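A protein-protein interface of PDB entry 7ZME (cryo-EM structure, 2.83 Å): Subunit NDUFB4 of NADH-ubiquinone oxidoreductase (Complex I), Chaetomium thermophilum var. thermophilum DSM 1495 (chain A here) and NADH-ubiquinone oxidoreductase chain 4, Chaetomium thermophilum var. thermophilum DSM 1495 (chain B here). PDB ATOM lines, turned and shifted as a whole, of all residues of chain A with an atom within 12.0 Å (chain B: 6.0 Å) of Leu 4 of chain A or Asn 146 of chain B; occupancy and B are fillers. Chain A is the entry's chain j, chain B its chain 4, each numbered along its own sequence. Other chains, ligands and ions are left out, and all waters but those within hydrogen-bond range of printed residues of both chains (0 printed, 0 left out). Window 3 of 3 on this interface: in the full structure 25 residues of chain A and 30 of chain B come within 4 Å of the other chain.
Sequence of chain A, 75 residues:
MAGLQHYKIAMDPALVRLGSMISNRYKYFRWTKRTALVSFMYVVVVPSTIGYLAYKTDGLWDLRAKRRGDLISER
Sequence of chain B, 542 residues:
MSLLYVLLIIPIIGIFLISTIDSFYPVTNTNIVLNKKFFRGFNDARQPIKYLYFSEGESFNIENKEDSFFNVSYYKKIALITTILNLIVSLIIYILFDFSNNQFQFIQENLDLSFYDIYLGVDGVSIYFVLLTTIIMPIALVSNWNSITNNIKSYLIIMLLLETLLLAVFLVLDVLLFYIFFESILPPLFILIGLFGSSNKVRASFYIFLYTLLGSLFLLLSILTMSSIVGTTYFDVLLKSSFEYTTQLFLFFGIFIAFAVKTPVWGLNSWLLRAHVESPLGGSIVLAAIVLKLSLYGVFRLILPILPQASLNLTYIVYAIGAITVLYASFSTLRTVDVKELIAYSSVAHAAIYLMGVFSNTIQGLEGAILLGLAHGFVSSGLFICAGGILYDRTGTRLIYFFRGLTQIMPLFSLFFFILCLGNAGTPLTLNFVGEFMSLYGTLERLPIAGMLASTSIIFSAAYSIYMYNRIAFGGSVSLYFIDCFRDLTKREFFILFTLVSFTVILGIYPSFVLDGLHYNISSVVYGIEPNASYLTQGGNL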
ATOM      1  N   GLY A   3      -4.519   1.764 -32.061  1.00  0.00           N
ATOM      2  CA  GLY A   3      -5.465   0.689 -32.291  1.00  0.00           C
ATOM      3  C   GLY A   3      -5.947   0.037 -31.011  1.00  0.00           C
ATOM      4  O   GLY A   3      -6.887   0.516 -30.377  1.00  0.00           O
ATOM      5  N   LEU A   4      -5.305  -1.065 -30.635  1.00  0.00           N
ATOM      6  CA  LEU A   4      -5.661  -1.757 -29.407  1.00  0.00           C
ATOM      7  C   LEU A   4      -5.359  -0.887 -28.192  1.00  0.00           C
ATOM      8  O   LEU A   4      -4.389  -0.124 -28.170  1.00  0.00           O
ATOM      9  CB  LEU A   4      -4.922  -3.095 -29.317  1.00  0.00           C
ATOM     10  CG  LEU A   4      -3.389  -3.135 -29.339  1.00  0.00           C
ATOM     11  CD1 LEU A   4      -2.776  -2.939 -27.956  1.00  0.00           C
ATOM     12  CD2 LEU A   4      -2.904  -4.439 -29.962  1.00  0.00           C
ATOM     13  N   GLN A   5      -6.212  -0.999 -27.180  1.00  0.00           N
ATOM     14  CA  GLN A   5      -6.051  -0.192 -25.981  1.00  0.00           C
ATOM     15  C   GLN A   5      -4.794  -0.597 -25.226  1.00  0.00           C
ATOM     16  O   GLN A   5      -4.363  -1.753 -25.258  1.00  0.00           O
ATOM     17  CB  GLN A   5      -7.277  -0.321 -25.078  1.00  0.00           C
ATOM     18  CG  GLN A   5      -7.494  -1.708 -24.503  1.00  0.00           C
ATOM     19  CD  GLN A   5      -8.756  -1.796 -23.669  1.00  0.00           C
ATOM     20  OE1 GLN A   5      -9.453  -0.801 -23.472  1.00  0.00           O
ATOM     21  NE2 GLN A   5      -9.057  -2.990 -23.173  1.00  0.00           N
ATOM     22  N   HIS A   6      -4.201   0.376 -24.545  1.00  0.00           N
ATOM     23  CA  HIS A   6      -2.974   0.193 -23.791  1.00  0.00           C
ATOM     24  C   HIS A   6      -3.268   0.299 -22.298  1.00  0.00           C
ATOM     25  O   HIS A   6      -4.416   0.428 -21.872  1.00  0.00           O
ATOM     26  CB  HIS A   6      -1.923   1.212 -24.231  1.00  0.00           C
ATOM     27  CG  HIS A   6      -2.382   2.633 -24.141  1.00  0.00           C
ATOM     28  ND1 HIS A   6      -2.213   3.399 -23.009  1.00  0.00           N
ATOM     29  CD2 HIS A   6      -2.998   3.429 -25.046  1.00  0.00           C
ATOM     30  CE1 HIS A   6      -2.709   4.605 -23.218  1.00  0.00           C
ATOM     31  NE2 HIS A   6      -3.193   4.649 -24.446  1.00  0.00           N
ATOM     32  N   TYR A   7      -2.208   0.233 -21.497  1.00  0.00           N
ATOM     33  CA  TYR A   7      -2.356   0.350 -20.058  1.00  0.00           C
ATOM     34  C   TYR A   7      -2.650   1.792 -19.672  1.00  0.00           C
ATOM     35  O   TYR A   7      -2.423   2.728 -20.442  1.00  0.00           O
ATOM     36  CB  TYR A   7      -1.096  -0.136 -19.345  1.00  0.00           C
ATOM     37  CG  TYR A   7      -0.982  -1.636 -19.269  1.00  0.00           C
ATOM     38  CD1 TYR A   7      -1.946  -2.388 -18.624  1.00  0.00           C
ATOM     39  CD2 TYR A   7       0.087  -2.300 -19.847  1.00  0.00           C
ATOM     40  CE1 TYR A   7      -1.851  -3.758 -18.557  1.00  0.00           C
ATOM     41  CE2 TYR A   7       0.196  -3.671 -19.778  1.00  0.00           C
ATOM     42  CZ  TYR A   7      -0.780  -4.395 -19.134  1.00  0.00           C
ATOM     43  OH  TYR A   7      -0.690  -5.763 -19.060  1.00  0.00           O
ATOM     44  N   LYS A   8      -3.165   1.967 -18.459  1.00  0.00           N
ATOM     45  CA  LYS A   8      -3.493   3.296 -17.962  1.00  0.00           C
ATOM     46  C   LYS A   8      -2.219   3.998 -17.510  1.00  0.00           C
ATOM     47  O   LYS A   8      -1.483   3.483 -16.663  1.00  0.00           O
ATOM     48  CB  LYS A   8      -4.508   3.210 -16.825  1.00  0.00           C
ATOM     49  CG  LYS A   8      -5.857   2.647 -17.254  1.00  0.00           C
ATOM     50  CD  LYS A   8      -6.859   2.647 -16.110  1.00  0.00           C
ATOM     51  CE  LYS A   8      -6.508   1.615 -15.053  1.00  0.00           C
ATOM     52  NZ  LYS A   8      -6.625   0.227 -15.575  1.00  0.00           N
ATOM     53  N   ILE A   9      -1.962   5.171 -18.082  1.00  0.00           N
ATOM     54  CA  ILE A   9      -0.741   5.930 -17.851  1.00  0.00           C
ATOM     55  C   ILE A   9      -1.119   7.257 -17.213  1.00  0.00           C
ATOM     56  O   ILE A   9      -2.032   7.940 -17.689  1.00  0.00           O
ATOM     57  CB  ILE A   9       0.038   6.154 -19.161  1.00  0.00           C
ATOM     58  CG1 ILE A   9       0.449   4.815 -19.774  1.00  0.00           C
ATOM     59  CG2 ILE A   9       1.258   7.048 -18.933  1.00  0.00           C
ATOM     60  CD1 ILE A   9       1.416   4.033 -18.934  1.00  0.00           C
ATOM     61  N   MET A  11      -0.693  10.402 -17.382  1.00  0.00           N
ATOM     62  CA  MET A  11      -0.150  11.300 -18.392  1.00  0.00           C
ATOM     63  C   MET A  11       0.073  12.676 -17.781  1.00  0.00           C
ATOM     64  O   MET A  11      -0.883  13.372 -17.429  1.00  0.00           O
ATOM     65  CB  MET A  11      -1.092  11.374 -19.587  1.00  0.00           C
ATOM     66  CG  MET A  11      -0.887  10.260 -20.589  1.00  0.00           C
ATOM     67  SD  MET A  11       0.800  10.178 -21.218  1.00  0.00           S
ATOM     68  CE  MET A  11       0.562   9.110 -22.633  1.00  0.00           C
ATOM     69  N   LYS B  76      -3.461 -13.258 -42.070  1.00  0.00           N
ATOM     70  CA  LYS B  76      -2.156 -13.178 -41.430  1.00  0.00           C
ATOM     71  C   LYS B  76      -1.426 -14.512 -41.489  1.00  0.00           C
ATOM     72  O   LYS B  76      -0.199 -14.539 -41.613  1.00  0.00           O
ATOM     73  CB  LYS B  76      -2.320 -12.705 -39.990  1.00  0.00           C
ATOM     74  CG  LYS B  76      -3.249 -11.524 -39.867  1.00  0.00           C
ATOM     75  CD  LYS B  76      -3.890 -11.448 -38.502  1.00  0.00           C
ATOM     76  CE  LYS B  76      -2.873 -11.152 -37.434  1.00  0.00           C
ATOM     77  NZ  LYS B  76      -3.527 -10.721 -36.171  1.00  0.00           N
ATOM     78  N   VAL B 142       5.009 -10.891 -37.982  1.00  0.00           N
ATOM     79  CA  VAL B 142       4.717 -11.408 -36.609  1.00  0.00           C
ATOM     80  C   VAL B 142       4.831 -10.266 -35.600  1.00  0.00           C
ATOM     81  O   VAL B 142       4.092 -10.286 -34.637  1.00  0.00           O
ATOM     82  CB  VAL B 142       5.636 -12.587 -36.254  1.00  0.00           C
ATOM     83  CG1 VAL B 142       5.333 -13.166 -34.884  1.00  0.00           C
ATOM     84  CG2 VAL B 142       5.578 -13.683 -37.297  1.00  0.00           C
ATOM     85  N   SER B 143       5.701  -9.286 -35.840  1.00  0.00           N
ATOM     86  CA  SER B 143       5.875  -8.109 -34.951  1.00  0.00           C
ATOM     87  C   SER B 143       4.598  -7.287 -34.884  1.00  0.00           C
ATOM     88  O   SER B 143       4.321  -6.731 -33.815  1.00  0.00           O
ATOM     89  CB  SER B 143       7.025  -7.268 -35.397  1.00  0.00           C
ATOM     90  OG  SER B 143       6.641  -6.382 -36.435  1.00  0.00           O
ATOM     91  N   ASN B 144       3.865  -7.190 -35.991  1.00  0.00           N
ATOM     92  CA  ASN B 144       2.652  -6.341 -36.055  1.00  0.00           C
ATOM     93  C   ASN B 144       1.402  -7.210 -36.012  1.00  0.00           C
ATOM     94  O   ASN B 144       0.354  -6.713 -36.431  1.00  0.00           O
ATOM     95  CB  ASN B 144       2.718  -5.387 -37.249  1.00  0.00           C
ATOM     96  CG  ASN B 144       2.774  -3.928 -36.856  1.00  0.00           C
ATOM     97  OD1 ASN B 144       2.768  -3.595 -35.676  1.00  0.00           O
ATOM     98  ND2 ASN B 144       2.824  -3.051 -37.838  1.00  0.00           N
ATOM     99  N   TRP B 145       1.497  -8.422 -35.463  1.00  0.00           N
ATOM    100  CA  TRP B 145       0.380  -9.399 -35.504  1.00  0.00           C
ATOM    101  C   TRP B 145      -0.873  -8.860 -34.817  1.00  0.00           C
ATOM    102  O   TRP B 145      -1.943  -9.016 -35.372  1.00  0.00           O
ATOM    103  CB  TRP B 145       0.845 -10.710 -34.871  1.00  0.00           C
ATOM    104  CG  TRP B 145       0.010 -11.919 -35.167  1.00  0.00           C
ATOM    105  CD1 TRP B 145      -1.002 -12.427 -34.406  1.00  0.00           C
ATOM    106  CD2 TRP B 145       0.149 -12.807 -36.290  1.00  0.00           C
ATOM    107  NE1 TRP B 145      -1.514 -13.555 -34.988  1.00  0.00           N
ATOM    108  CE2 TRP B 145      -0.831 -13.811 -36.144  1.00  0.00           C
ATOM    109  CE3 TRP B 145       0.993 -12.848 -37.403  1.00  0.00           C
ATOM    110  CZ2 TRP B 145      -0.989 -14.836 -37.073  1.00  0.00           C
ATOM    111  CZ3 TRP B 145       0.837 -13.861 -38.318  1.00  0.00           C
ATOM    112  CH2 TRP B 145      -0.136 -14.845 -38.151  1.00  0.00           C
ATOM    113  N   ASN B 146      -0.742  -8.196 -33.681  1.00  0.00           N
ATOM    114  CA  ASN B 146      -1.954  -7.789 -32.943  1.00  0.00           C
ATOM    115  C   ASN B 146      -2.184  -6.293 -33.120  1.00  0.00           C
ATOM    116  O   ASN B 146      -3.339  -5.880 -33.039  1.00  0.00           O
ATOM    117  CB  ASN B 146      -1.822  -8.270 -31.500  1.00  0.00           C
ATOM    118  CG  ASN B 146      -1.706  -9.771 -31.365  1.00  0.00           C
ATOM    119  OD1 ASN B 146      -2.525 -10.514 -31.899  1.00  0.00           O
ATOM    120  ND2 ASN B 146      -0.703 -10.227 -30.636  1.00  0.00           N
ATOM    121  N   SER B 147      -1.143  -5.528 -33.429  1.00  0.00           N
ATOM    122  CA  SER B 147      -1.235  -4.049 -33.533  1.00  0.00           C
ATOM    123  C   SER B 147      -2.050  -3.550 -34.730  1.00  0.00           C
ATOM    124  O   SER B 147      -2.683  -2.492 -34.591  1.00  0.00           O
ATOM    125  CB  SER B 147       0.129  -3.450 -33.498  1.00  0.00           C
ATOM    126  OG  SER B 147       0.864  -3.942 -32.390  1.00  0.00           O
ATOM    127  N   ILE B 148      -2.014  -4.245 -35.863  1.00  0.00           N
ATOM    128  CA  ILE B 148      -2.822  -3.847 -37.010  1.00  0.00           C
ATOM    129  C   ILE B 148      -4.249  -4.308 -36.743  1.00  0.00           C
ATOM    130  O   ILE B 148      -4.525  -5.508 -36.699  1.00  0.00           O
ATOM    131  CB  ILE B 148      -2.286  -4.433 -38.322  1.00  0.00           C
ATOM    132  CG1 ILE B 148      -0.850  -3.972 -38.577  1.00  0.00           C
ATOM    133  CG2 ILE B 148      -3.183  -4.049 -39.486  1.00  0.00           C
ATOM    134  CD1 ILE B 148      -0.699  -2.483 -38.704  1.00  0.00           C
ATOM    135  N   THR B 149      -5.163  -3.353 -36.571  1.00  0.00           N
ATOM    136  CA  THR B 149      -6.542  -3.664 -36.232  1.00  0.00           C
ATOM    137  C   THR B 149      -7.533  -3.363 -37.345  1.00  0.00           C
ATOM    138  O   THR B 149      -8.646  -3.895 -37.314  1.00  0.00           O
ATOM    139  CB  THR B 149      -6.969  -2.897 -34.974  1.00  0.00           C
ATOM    140  OG1 THR B 149      -6.887  -1.488 -35.222  1.00  0.00           O
ATOM    141  CG2 THR B 149      -6.064  -3.250 -33.805  1.00  0.00           C
ATOM    142  N   ASP B 393       3.112  -0.082 -27.396  1.00  0.00           N
ATOM    143  CA  ASP B 393       1.825  -0.763 -27.333  1.00  0.00           C
ATOM    144  C   ASP B 393       1.290  -0.835 -25.912  1.00  0.00           C
ATOM    145  O   ASP B 393       0.073  -0.915 -25.716  1.00  0.00           O
ATOM    146  CB  ASP B 393       1.936  -2.164 -27.933  1.00  0.00           C
ATOM    147  CG  ASP B 393       1.812  -2.157 -29.441  1.00  0.00           C
ATOM    148  OD1 ASP B 393       0.877  -1.509 -29.955  1.00  0.00           O
ATOM    149  OD2 ASP B 393       2.641  -2.797 -30.118  1.00  0.00           O
ATOM    150  N   ARG B 492       5.256 -14.157 -28.356  1.00  0.00           N
ATOM    151  CA  ARG B 492       5.546 -13.546 -29.679  1.00  0.00           C
ATOM    152  C   ARG B 492       6.634 -12.492 -29.537  1.00  0.00           C
ATOM    153  O   ARG B 492       7.584 -12.512 -30.334  1.00  0.00           O
ATOM    154  CB  ARG B 492       4.286 -12.905 -30.250  1.00  0.00           C
ATOM    155  CG  ARG B 492       4.435 -12.313 -31.638  1.00  0.00           C
ATOM    156  CD  ARG B 492       3.135 -11.649 -32.044  1.00  0.00           C
ATOM    157  NE  ARG B 492       2.739 -10.601 -31.118  1.00  0.00           N
ATOM    158  CZ  ARG B 492       3.225  -9.369 -31.119  1.00  0.00           C
ATOM    159  NH1 ARG B 492       2.803  -8.491 -30.227  1.00  0.00           N
ATOM    160  NH2 ARG B 492       4.146  -9.019 -31.996  1.00  0.00           N
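The guanidinium group (NE) of Arg 492 of chain B lies close to the side-chain amide nitrogen (ND2) of Asn 146 of chain B, at 3.5 Å.
OD2 of Asp 393 of chain B lies within hydrogen-bond range of OG of Ser 147 of chain B (3.1 Å).
Among the printed residues, pairs that only touch across the chains: His 6 of chain A with Asp 393 of chain B (3.3 Å), Leu 4 of chain A with Asn 146 of chain B (3.4 Å), Gly 3 of chain A with Thr 149 of chain B (3.9 Å), Leu 4 of chain A with Thr 149 of chain B (3.9 Å) and Leu 4 of chain A with Ser 147 of chain B (3.96 Å).
Printed residues of chain B within 4 Å of Gly 3 of chain A: Thr 149 (3.9 Å).
Of chain B, only Asn 146 (3.4 Å), Ser 147 (3.96 Å) and Thr 149 (3.9 Å) come within 4 Å of Leu 4 of chain A.
Printed residues of chain B within 4 Å of His 6 of chain A: Asp 393.
Ile 9 of chain A touches none of the printed residues of chain B.
Asn 144 of chain B touches none of the printed residues of chain A.
Asn 146 of chain B touches just one residue of chain A: Leu 4 (3.4 Å).
Of chain A, only Leu 4 (3.96 Å) comes within 4 Å of Ser 147 of chain B.
No residue of chain A comes within 4 Å of Ile 148 of chain B.
Of chain A, only His 6 (3.3 Å) comes within 4 Å of Asp 393 of chain B.
The nearest printed residue of chain B that does not touch His 6 of chain A is Ser 147 of chain B (10.0 Å).
Of the 8 printed residues of chain A, 3 touch a printed residue of chain B.
Printed residues of chain A that touch a printed residue of chain B: Gly 3, Leu 4 and His 6.
Hydrophobic or aromatic side chains of chain A that line the printed part of chain B: Leu 4 and His 6.
Among the printed residues, 5 pairs touch across the chains.
Among the printed residues, no Asp or Glu carboxylate lies within 4 Å of a Lys or Arg side-chain nitrogen of the other chain.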
